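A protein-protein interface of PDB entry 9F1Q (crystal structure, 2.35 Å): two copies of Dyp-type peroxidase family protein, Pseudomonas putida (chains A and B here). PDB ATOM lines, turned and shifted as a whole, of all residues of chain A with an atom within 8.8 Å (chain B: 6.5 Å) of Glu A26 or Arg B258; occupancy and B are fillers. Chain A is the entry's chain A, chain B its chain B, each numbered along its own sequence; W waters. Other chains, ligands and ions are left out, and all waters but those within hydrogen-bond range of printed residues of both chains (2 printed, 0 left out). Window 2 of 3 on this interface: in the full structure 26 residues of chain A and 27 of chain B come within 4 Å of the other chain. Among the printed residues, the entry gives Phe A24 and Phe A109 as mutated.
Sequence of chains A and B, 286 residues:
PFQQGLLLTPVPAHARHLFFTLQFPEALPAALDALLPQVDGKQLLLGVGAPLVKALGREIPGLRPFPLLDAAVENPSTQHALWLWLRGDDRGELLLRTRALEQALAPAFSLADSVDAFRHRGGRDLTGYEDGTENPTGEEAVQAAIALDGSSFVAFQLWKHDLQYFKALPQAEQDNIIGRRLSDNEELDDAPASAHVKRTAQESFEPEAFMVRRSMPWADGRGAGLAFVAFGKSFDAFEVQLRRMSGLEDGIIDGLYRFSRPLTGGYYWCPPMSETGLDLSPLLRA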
ATOM      1  N   LEU A  22      -9.405  25.202 -23.199  1.00  0.00           N
ATOM      2  CA  LEU A  22      -8.042  24.975 -23.673  1.00  0.00           C
ATOM      3  C   LEU A  22      -7.552  23.695 -23.011  1.00  0.00           C
ATOM      4  O   LEU A  22      -7.028  23.700 -21.896  1.00  0.00           O
ATOM      5  CB  LEU A  22      -7.140  26.159 -23.357  1.00  0.00           C
ATOM      6  CG  LEU A  22      -5.739  26.045 -23.961  1.00  0.00           C
ATOM      7  CD1 LEU A  22      -5.817  25.924 -25.480  1.00  0.00           C
ATOM      8  CD2 LEU A  22      -4.887  27.232 -23.560  1.00  0.00           C
ATOM      9  N   GLN A  23      -7.718  22.578 -23.719  1.00  0.00           N
ATOM     10  CA  GLN A  23      -7.389  21.280 -23.141  1.00  0.00           C
ATOM     11  C   GLN A  23      -5.908  20.954 -23.281  1.00  0.00           C
ATOM     12  O   GLN A  23      -5.313  20.371 -22.369  1.00  0.00           O
ATOM     13  CB  GLN A  23      -8.241  20.190 -23.791  1.00  0.00           C
ATOM     14  CG  GLN A  23      -8.038  18.797 -23.208  1.00  0.00           C
ATOM     15  CD  GLN A  23      -8.109  18.768 -21.693  1.00  0.00           C
ATOM     16  OE1 GLN A  23      -8.919  19.464 -21.078  1.00  0.00           O
ATOM     17  NE2 GLN A  23      -7.256  17.955 -21.082  1.00  0.00           N
ATOM     18  N   PHE A  24      -5.298  21.298 -24.415  1.00  0.00           N
ATOM     19  CA  PHE A  24      -3.882  21.027 -24.655  1.00  0.00           C
ATOM     20  C   PHE A  24      -3.231  22.315 -25.136  1.00  0.00           C
ATOM     21  O   PHE A  24      -3.150  22.573 -26.346  1.00  0.00           O
ATOM     22  CB  PHE A  24      -3.710  19.881 -25.648  1.00  0.00           C
ATOM     23  CG  PHE A  24      -4.269  18.576 -25.156  1.00  0.00           C
ATOM     24  CD1 PHE A  24      -3.695  17.924 -24.076  1.00  0.00           C
ATOM     25  CD2 PHE A  24      -5.385  18.012 -25.755  1.00  0.00           C
ATOM     26  CE1 PHE A  24      -4.214  16.727 -23.614  1.00  0.00           C
ATOM     27  CE2 PHE A  24      -5.908  16.817 -25.299  1.00  0.00           C
ATOM     28  CZ  PHE A  24      -5.322  16.173 -24.226  1.00  0.00           C
ATOM     29  N   PRO A  25      -2.752  23.150 -24.212  1.00  0.00           N
ATOM     30  CA  PRO A  25      -2.222  24.465 -24.608  1.00  0.00           C
ATOM     31  C   PRO A  25      -0.990  24.392 -25.490  1.00  0.00           C
ATOM     32  O   PRO A  25      -0.706  25.361 -26.204  1.00  0.00           O
ATOM     33  CB  PRO A  25      -1.915  25.146 -23.267  1.00  0.00           C
ATOM     34  CG  PRO A  25      -1.812  24.037 -22.274  1.00  0.00           C
ATOM     35  CD  PRO A  25      -2.707  22.939 -22.755  1.00  0.00           C
ATOM     36  N   GLU A  26      -0.239  23.288 -25.456  1.00  0.00           N
ATOM     37  CA  GLU A  26       0.920  23.164 -26.330  1.00  0.00           C
ATOM     38  C   GLU A  26       0.522  23.082 -27.795  1.00  0.00           C
ATOM     39  O   GLU A  26       1.336  23.409 -28.664  1.00  0.00           O
ATOM     40  CB  GLU A  26       1.753  21.936 -25.953  1.00  0.00           C
ATOM     41  CG  GLU A  26       1.059  20.600 -26.174  1.00  0.00           C
ATOM     42  CD  GLU A  26       0.221  20.172 -24.986  1.00  0.00           C
ATOM     43  OE1 GLU A  26      -0.049  21.019 -24.107  1.00  0.00           O
ATOM     44  OE2 GLU A  26      -0.161  18.986 -24.924  1.00  0.00           O
ATOM     45  N   ALA A  27      -0.710  22.667 -28.083  1.00  0.00           N
ATOM     46  CA  ALA A  27      -1.222  22.573 -29.443  1.00  0.00           C
ATOM     47  C   ALA A  27      -1.932  23.844 -29.890  1.00  0.00           C
ATOM     48  O   ALA A  27      -2.600  23.833 -30.928  1.00  0.00           O
ATOM     49  CB  ALA A  27      -2.166  21.376 -29.569  1.00  0.00           C
ATOM     50  N   LEU A  28      -1.803  24.930 -29.128  1.00  0.00           N
ATOM     51  CA  LEU A  28      -2.468  26.181 -29.484  1.00  0.00           C
ATOM     52  C   LEU A  28      -2.057  26.756 -30.839  1.00  0.00           C
ATOM     53  O   LEU A  28      -2.944  27.271 -31.545  1.00  0.00           O
ATOM     54  CB  LEU A  28      -2.228  27.218 -28.379  1.00  0.00           C
ATOM     55  CG  LEU A  28      -2.935  28.567 -28.548  1.00  0.00           C
ATOM     56  CD1 LEU A  28      -4.436  28.383 -28.690  1.00  0.00           C
ATOM     57  CD2 LEU A  28      -2.613  29.495 -27.387  1.00  0.00           C
ATOM     58  N   PRO A  29      -0.780  26.730 -31.260  1.00  0.00           N
ATOM     59  CA  PRO A  29      -0.431  27.383 -32.538  1.00  0.00           C
ATOM     60  C   PRO A  29      -1.206  26.870 -33.741  1.00  0.00           C
ATOM     61  O   PRO A  29      -1.650  27.678 -34.567  1.00  0.00           O
ATOM     62  CB  PRO A  29       1.071  27.098 -32.669  1.00  0.00           C
ATOM     63  CG  PRO A  29       1.541  26.969 -31.273  1.00  0.00           C
ATOM     64  CD  PRO A  29       0.429  26.272 -30.547  1.00  0.00           C
ATOM     65  N   ALA A  30      -1.383  25.554 -33.872  1.00  0.00           N
ATOM     66  CA  ALA A  30      -2.127  25.023 -35.011  1.00  0.00           C
ATOM     67  C   ALA A  30      -3.584  25.472 -34.979  1.00  0.00           C
ATOM     68  O   ALA A  30      -4.183  25.737 -36.029  1.00  0.00           O
ATOM     69  CB  ALA A  30      -2.037  23.498 -35.037  1.00  0.00           C
ATOM     70  N   ALA A  31      -4.171  25.565 -33.782  1.00  0.00           N
ATOM     71  CA  ALA A  31      -5.556  26.008 -33.660  1.00  0.00           C
ATOM     72  C   ALA A  31      -5.712  27.464 -34.085  1.00  0.00           C
ATOM     73  O   ALA A  31      -6.651  27.811 -34.809  1.00  0.00           O
ATOM     74  CB  ALA A  31      -6.045  25.806 -32.225  1.00  0.00           C
ATOM     75  N   ALA A  55      -2.784  30.774 -19.351  1.00  0.00           N
ATOM     76  CA  ALA A  55      -2.003  29.669 -19.894  1.00  0.00           C
ATOM     77  C   ALA A  55      -0.809  30.168 -20.697  1.00  0.00           C
ATOM     78  O   ALA A  55       0.207  29.470 -20.790  1.00  0.00           O
ATOM     79  CB  ALA A  55      -2.887  28.772 -20.761  1.00  0.00           C
ATOM     80  N   LEU A  56      -0.910  31.360 -21.282  1.00  0.00           N
ATOM     81  CA  LEU A  56       0.203  31.974 -21.994  1.00  0.00           C
ATOM     82  C   LEU A  56       1.084  32.829 -21.093  1.00  0.00           C
ATOM     83  O   LEU A  56       2.028  33.453 -21.588  1.00  0.00           O
ATOM     84  CB  LEU A  56      -0.320  32.824 -23.157  1.00  0.00           C
ATOM     85  CG  LEU A  56      -1.007  32.060 -24.290  1.00  0.00           C
ATOM     86  CD1 LEU A  56      -1.509  33.020 -25.355  1.00  0.00           C
ATOM     87  CD2 LEU A  56      -0.063  31.029 -24.889  1.00  0.00           C
ATOM     88  N   PRO A 107      -6.548  19.320 -31.435  1.00  0.00           N
ATOM     89  CA  PRO A 107      -6.884  18.905 -30.065  1.00  0.00           C
ATOM     90  C   PRO A 107      -6.659  19.985 -29.011  1.00  0.00           C
ATOM     91  O   PRO A 107      -6.939  19.757 -27.836  1.00  0.00           O
ATOM     92  CB  PRO A 107      -5.943  17.716 -29.849  1.00  0.00           C
ATOM     93  CG  PRO A 107      -4.695  18.130 -30.593  1.00  0.00           C
ATOM     94  CD  PRO A 107      -5.189  18.885 -31.813  1.00  0.00           C
ATOM     95  N   ALA A 108      -6.137  21.155 -29.396  1.00  0.00           N
ATOM     96  CA  ALA A 108      -5.866  22.212 -28.424  1.00  0.00           C
ATOM     97  C   ALA A 108      -7.122  22.596 -27.650  1.00  0.00           C
ATOM     98  O   ALA A 108      -7.095  22.725 -26.421  1.00  0.00           O
ATOM     99  CB  ALA A 108      -5.276  23.434 -29.126  1.00  0.00           C
ATOM    100  N   PHE A 109      -8.235  22.780 -28.355  1.00  0.00           N
ATOM    101  CA  PHE A 109      -9.482  23.234 -27.758  1.00  0.00           C
ATOM    102  C   PHE A 109     -10.508  22.109 -27.753  1.00  0.00           C
ATOM    103  O   PHE A 109     -10.616  21.346 -28.719  1.00  0.00           O
ATOM    104  CB  PHE A 109     -10.052  24.442 -28.509  1.00  0.00           C
ATOM    105  CG  PHE A 109      -9.319  25.723 -28.244  1.00  0.00           C
ATOM    106  CD1 PHE A 109      -9.502  26.406 -27.050  1.00  0.00           C
ATOM    107  CD2 PHE A 109      -8.450  26.249 -29.185  1.00  0.00           C
ATOM    108  CE1 PHE A 109      -8.831  27.587 -26.798  1.00  0.00           C
ATOM    109  CE2 PHE A 109      -7.775  27.431 -28.940  1.00  0.00           C
ATOM    110  CZ  PHE A 109      -7.964  28.100 -27.747  1.00  0.00           C
ATOM    111  N   ASP B 162     -11.881  12.021 -19.714  1.00  0.00           N
ATOM    112  CA  ASP B 162     -11.684  11.609 -21.104  1.00  0.00           C
ATOM    113  C   ASP B 162     -10.961  10.265 -21.063  1.00  0.00           C
ATOM    114  O   ASP B 162      -9.737  10.178 -21.163  1.00  0.00           O
ATOM    115  CB  ASP B 162     -10.909  12.667 -21.886  1.00  0.00           C
ATOM    116  CG  ASP B 162     -10.811  12.346 -23.374  1.00  0.00           C
ATOM    117  OD1 ASP B 162     -11.168  11.218 -23.780  1.00  0.00           O
ATOM    118  OD2 ASP B 162     -10.382  13.230 -24.144  1.00  0.00           O
ATOM    119  N   TYR B 165      -8.764   9.118 -24.284  1.00  0.00           N
ATOM    120  CA  TYR B 165      -7.431   9.706 -24.326  1.00  0.00           C
ATOM    121  C   TYR B 165      -6.530   9.100 -23.258  1.00  0.00           C
ATOM    122  O   TYR B 165      -5.395   8.699 -23.541  1.00  0.00           O
ATOM    123  CB  TYR B 165      -7.519  11.222 -24.158  1.00  0.00           C
ATOM    124  CG  TYR B 165      -6.186  11.860 -23.842  1.00  0.00           C
ATOM    125  CD1 TYR B 165      -5.236  12.054 -24.835  1.00  0.00           C
ATOM    126  CD2 TYR B 165      -5.877  12.263 -22.549  1.00  0.00           C
ATOM    127  CE1 TYR B 165      -4.012  12.631 -24.550  1.00  0.00           C
ATOM    128  CE2 TYR B 165      -4.658  12.841 -22.254  1.00  0.00           C
ATOM    129  CZ  TYR B 165      -3.730  13.023 -23.259  1.00  0.00           C
ATOM    130  OH  TYR B 165      -2.513  13.600 -22.972  1.00  0.00           O
ATOM    131  N   PHE B 166      -7.018   9.039 -22.017  1.00  0.00           N
ATOM    132  CA  PHE B 166      -6.177   8.625 -20.899  1.00  0.00           C
ATOM    133  C   PHE B 166      -5.740   7.171 -21.036  1.00  0.00           C
ATOM    134  O   PHE B 166      -4.552   6.856 -20.901  1.00  0.00           O
ATOM    135  CB  PHE B 166      -6.920   8.843 -19.581  1.00  0.00           C
ATOM    136  CG  PHE B 166      -6.104   8.521 -18.365  1.00  0.00           C
ATOM    137  CD1 PHE B 166      -5.140   9.406 -17.907  1.00  0.00           C
ATOM    138  CD2 PHE B 166      -6.297   7.333 -17.677  1.00  0.00           C
ATOM    139  CE1 PHE B 166      -4.386   9.116 -16.785  1.00  0.00           C
ATOM    140  CE2 PHE B 166      -5.545   7.035 -16.555  1.00  0.00           C
ATOM    141  CZ  PHE B 166      -4.587   7.928 -16.108  1.00  0.00           C
ATOM    142  N   LEU B 169      -2.901   6.275 -23.372  1.00  0.00           N
ATOM    143  CA  LEU B 169      -1.543   6.638 -23.013  1.00  0.00           C
ATOM    144  C   LEU B 169      -0.756   5.396 -22.599  1.00  0.00           C
ATOM    145  O   LEU B 169      -1.335   4.414 -22.124  1.00  0.00           O
ATOM    146  CB  LEU B 169      -1.542   7.643 -21.864  1.00  0.00           C
ATOM    147  CG  LEU B 169      -2.119   9.041 -22.099  1.00  0.00           C
ATOM    148  CD1 LEU B 169      -2.206   9.796 -20.780  1.00  0.00           C
ATOM    149  CD2 LEU B 169      -1.293   9.814 -23.113  1.00  0.00           C
ATOM    150  N   ILE B 177       0.826  10.603 -14.238  1.00  0.00           N
ATOM    151  CA  ILE B 177      -0.247  11.561 -13.996  1.00  0.00           C
ATOM    152  C   ILE B 177      -0.847  11.358 -12.608  1.00  0.00           C
ATOM    153  O   ILE B 177      -1.082  12.324 -11.873  1.00  0.00           O
ATOM    154  CB  ILE B 177      -1.310  11.458 -15.104  1.00  0.00           C
ATOM    155  CG1 ILE B 177      -0.818  12.168 -16.368  1.00  0.00           C
ATOM    156  CG2 ILE B 177      -2.643  12.020 -14.636  1.00  0.00           C
ATOM    157  CD1 ILE B 177      -1.676  11.919 -17.583  1.00  0.00           C
ATOM    158  N   ASP B 254      -1.681  20.284 -11.906  1.00  0.00           N
ATOM    159  CA  ASP B 254      -1.873  18.860 -11.662  1.00  0.00           C
ATOM    160  C   ASP B 254      -2.090  18.112 -12.972  1.00  0.00           C
ATOM    161  O   ASP B 254      -2.716  18.621 -13.906  1.00  0.00           O
ATOM    162  CB  ASP B 254      -3.065  18.650 -10.722  1.00  0.00           C
ATOM    163  CG  ASP B 254      -3.155  17.229 -10.184  1.00  0.00           C
ATOM    164  OD1 ASP B 254      -3.041  16.269 -10.975  1.00  0.00           O
ATOM    165  OD2 ASP B 254      -3.344  17.074  -8.960  1.00  0.00           O
ATOM    166  N   GLY B 255      -1.563  16.886 -13.035  1.00  0.00           N
ATOM    167  CA  GLY B 255      -1.699  16.065 -14.224  1.00  0.00           C
ATOM    168  C   GLY B 255      -3.111  15.598 -14.510  1.00  0.00           C
ATOM    169  O   GLY B 255      -3.397  15.191 -15.642  1.00  0.00           O
ATOM    170  N   LEU B 256      -3.998  15.632 -13.510  1.00  0.00           N
ATOM    171  CA  LEU B 256      -5.384  15.226 -13.736  1.00  0.00           C
ATOM    172  C   LEU B 256      -6.045  16.065 -14.819  1.00  0.00           C
ATOM    173  O   LEU B 256      -6.875  15.553 -15.579  1.00  0.00           O
ATOM    174  CB  LEU B 256      -6.191  15.325 -12.441  1.00  0.00           C
ATOM    175  CG  LEU B 256      -5.882  14.349 -11.307  1.00  0.00           C
ATOM    176  CD1 LEU B 256      -6.933  14.494 -10.227  1.00  0.00           C
ATOM    177  CD2 LEU B 256      -5.825  12.917 -11.813  1.00  0.00           C
ATOM    178  N   TYR B 257      -5.701  17.353 -14.902  1.00  0.00           N
ATOM    179  CA  TYR B 257      -6.307  18.231 -15.896  1.00  0.00           C
ATOM    180  C   TYR B 257      -5.913  17.872 -17.323  1.00  0.00           C
ATOM    181  O   TYR B 257      -6.456  18.465 -18.261  1.00  0.00           O
ATOM    182  CB  TYR B 257      -5.942  19.687 -15.609  1.00  0.00           C
ATOM    183  CG  TYR B 257      -6.579  20.247 -14.356  1.00  0.00           C
ATOM    184  CD1 TYR B 257      -7.913  20.635 -14.346  1.00  0.00           C
ATOM    185  CD2 TYR B 257      -5.844  20.401 -13.188  1.00  0.00           C
ATOM    186  CE1 TYR B 257      -8.500  21.149 -13.206  1.00  0.00           C
ATOM    187  CE2 TYR B 257      -6.422  20.917 -12.041  1.00  0.00           C
ATOM    188  CZ  TYR B 257      -7.752  21.288 -12.058  1.00  0.00           C
ATOM    189  OH  TYR B 257      -8.335  21.802 -10.923  1.00  0.00           O
ATOM    190  N   ARG B 258      -4.986  16.928 -17.514  1.00  0.00           N
ATOM    191  CA  ARG B 258      -4.686  16.459 -18.861  1.00  0.00           C
ATOM    192  C   ARG B 258      -5.839  15.645 -19.435  1.00  0.00           C
ATOM    193  O   ARG B 258      -6.036  15.631 -20.655  1.00  0.00           O
ATOM    194  CB  ARG B 258      -3.396  15.633 -18.868  1.00  0.00           C
ATOM    195  CG  ARG B 258      -2.147  16.386 -18.420  1.00  0.00           C
ATOM    196  CD  ARG B 258      -1.712  17.460 -19.417  1.00  0.00           C
ATOM    197  NE  ARG B 258      -1.222  16.909 -20.677  1.00  0.00           N
ATOM    198  CZ  ARG B 258      -0.879  17.640 -21.729  1.00  0.00           C
ATOM    199  NH1 ARG B 258      -0.969  18.960 -21.713  1.00  0.00           N
ATOM    200  NH2 ARG B 258      -0.433  17.032 -22.826  1.00  0.00           N
ATOM    201  N   PHE B 259      -6.609  14.962 -18.580  1.00  0.00           N
ATOM    202  CA  PHE B 259      -7.667  14.078 -19.047  1.00  0.00           C
ATOM    203  C   PHE B 259      -9.009  14.286 -18.357  1.00  0.00           C
ATOM    204  O   PHE B 259      -9.986  13.633 -18.741  1.00  0.00           O
ATOM    205  CB  PHE B 259      -7.238  12.608 -18.889  1.00  0.00           C
ATOM    206  CG  PHE B 259      -7.323  12.089 -17.477  1.00  0.00           C
ATOM    207  CD1 PHE B 259      -6.312  12.347 -16.563  1.00  0.00           C
ATOM    208  CD2 PHE B 259      -8.403  11.320 -17.072  1.00  0.00           C
ATOM    209  CE1 PHE B 259      -6.386  11.864 -15.267  1.00  0.00           C
ATOM    210  CE2 PHE B 259      -8.484  10.835 -15.778  1.00  0.00           C
ATOM    211  CZ  PHE B 259      -7.474  11.106 -14.875  1.00  0.00           C
ATOM    212  N   SER B 260      -9.093  15.161 -17.356  1.00  0.00           N
ATOM    213  CA  SER B 260     -10.328  15.359 -16.608  1.00  0.00           C
ATOM    214  C   SER B 260     -10.495  16.835 -16.277  1.00  0.00           C
ATOM    215  O   SER B 260      -9.514  17.573 -16.156  1.00  0.00           O
ATOM    216  CB  SER B 260     -10.347  14.523 -15.318  1.00  0.00           C
ATOM    217  OG  SER B 260     -11.637  14.513 -14.728  1.00  0.00           O
HETATM  218  O   HOH W   1      -8.099  15.123 -22.285  1.00  0.00           O
HETATM  219  O   HOH W   2      -8.934  20.515 -18.081  1.00  0.00           O
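The side-chain amide nitrogen (NE2) of Gln A23 lies within hydrogen-bond range of the backbone carbonyl oxygen (O) of Tyr B257, 3.0 Å away.
NE2 of Gln A23 is in hydrogen-bond range of O of Arg B258 (2.7 Å).
The side-chain carboxylate (OE2) of Glu A26 is in salt-bridge range of the guanidinium group (NH2) of Arg B258.
The backbone NH of Phe A24 lies within hydrogen-bond range of the backbone carbonyl oxygen of Ala A108.
N of Asp B162 lies within hydrogen-bond range of O of Phe B259.
The backbone NH of Gln A23 lies within hydrogen-bond range of the backbone carbonyl oxygen of Ala A108, 2.8 Å away.
The backbone NH (N) of Tyr B165 sits at hydrogen-bond distance from the side-chain carboxylate (OD1) of Asp B162, at 3.2 Å.
Among the printed residues, merely in contact across the chains: Phe A24 with Arg B258 (3.6 Å), Phe A24 with Tyr B165 (3.6 Å) and Gln A23 with Phe B259 (3.95 Å).
Of the printed residues of chain B, Gln A23 touches Tyr B257, Arg B258 and Phe B259.
Of the printed residues of chain B, Phe A24 touches Tyr B165 and Arg B258.
Printed residues of chain B within 4 Å of Glu A26: Arg B258 (2.9 Å).
Ala A55 touches none of the printed residues of chain B.
Printed residues of chain A within 4 Å of Tyr B165: Phe A24.
Printed residues of chain A within 4 Å of Tyr B257: Gln A23.
Arg B258 touches just these residues of chain A: Gln A23, Phe A24 and Glu A26.
Of the printed residues of chain A, Phe B259 touches Gln A23.
The nearest printed residue of chain B that does not touch Gln A23 is Ser B260 (5.0 Å).
Of the 12 printed residues of chain B, 4 touch a printed residue of chain A.
Printed residues of chain B that touch a printed residue of chain A: Tyr B165, Tyr B257, Arg B258 and Phe B259.
Of the 15 printed residues of chain A, 3 touch a printed residue of chain B.
Among the printed residues, Asp or Glu carboxylates within 4 Å of a Lys or Arg side-chain nitrogen of the other chain: Glu A26 with Arg B258 (2.9 Å).
No position is printed for both chains.
Water W2 bridges the side-chain amide oxygen of Gln A23 (3.2 Å) and the backbone carbonyl oxygen of Tyr B257 (3.2 Å).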
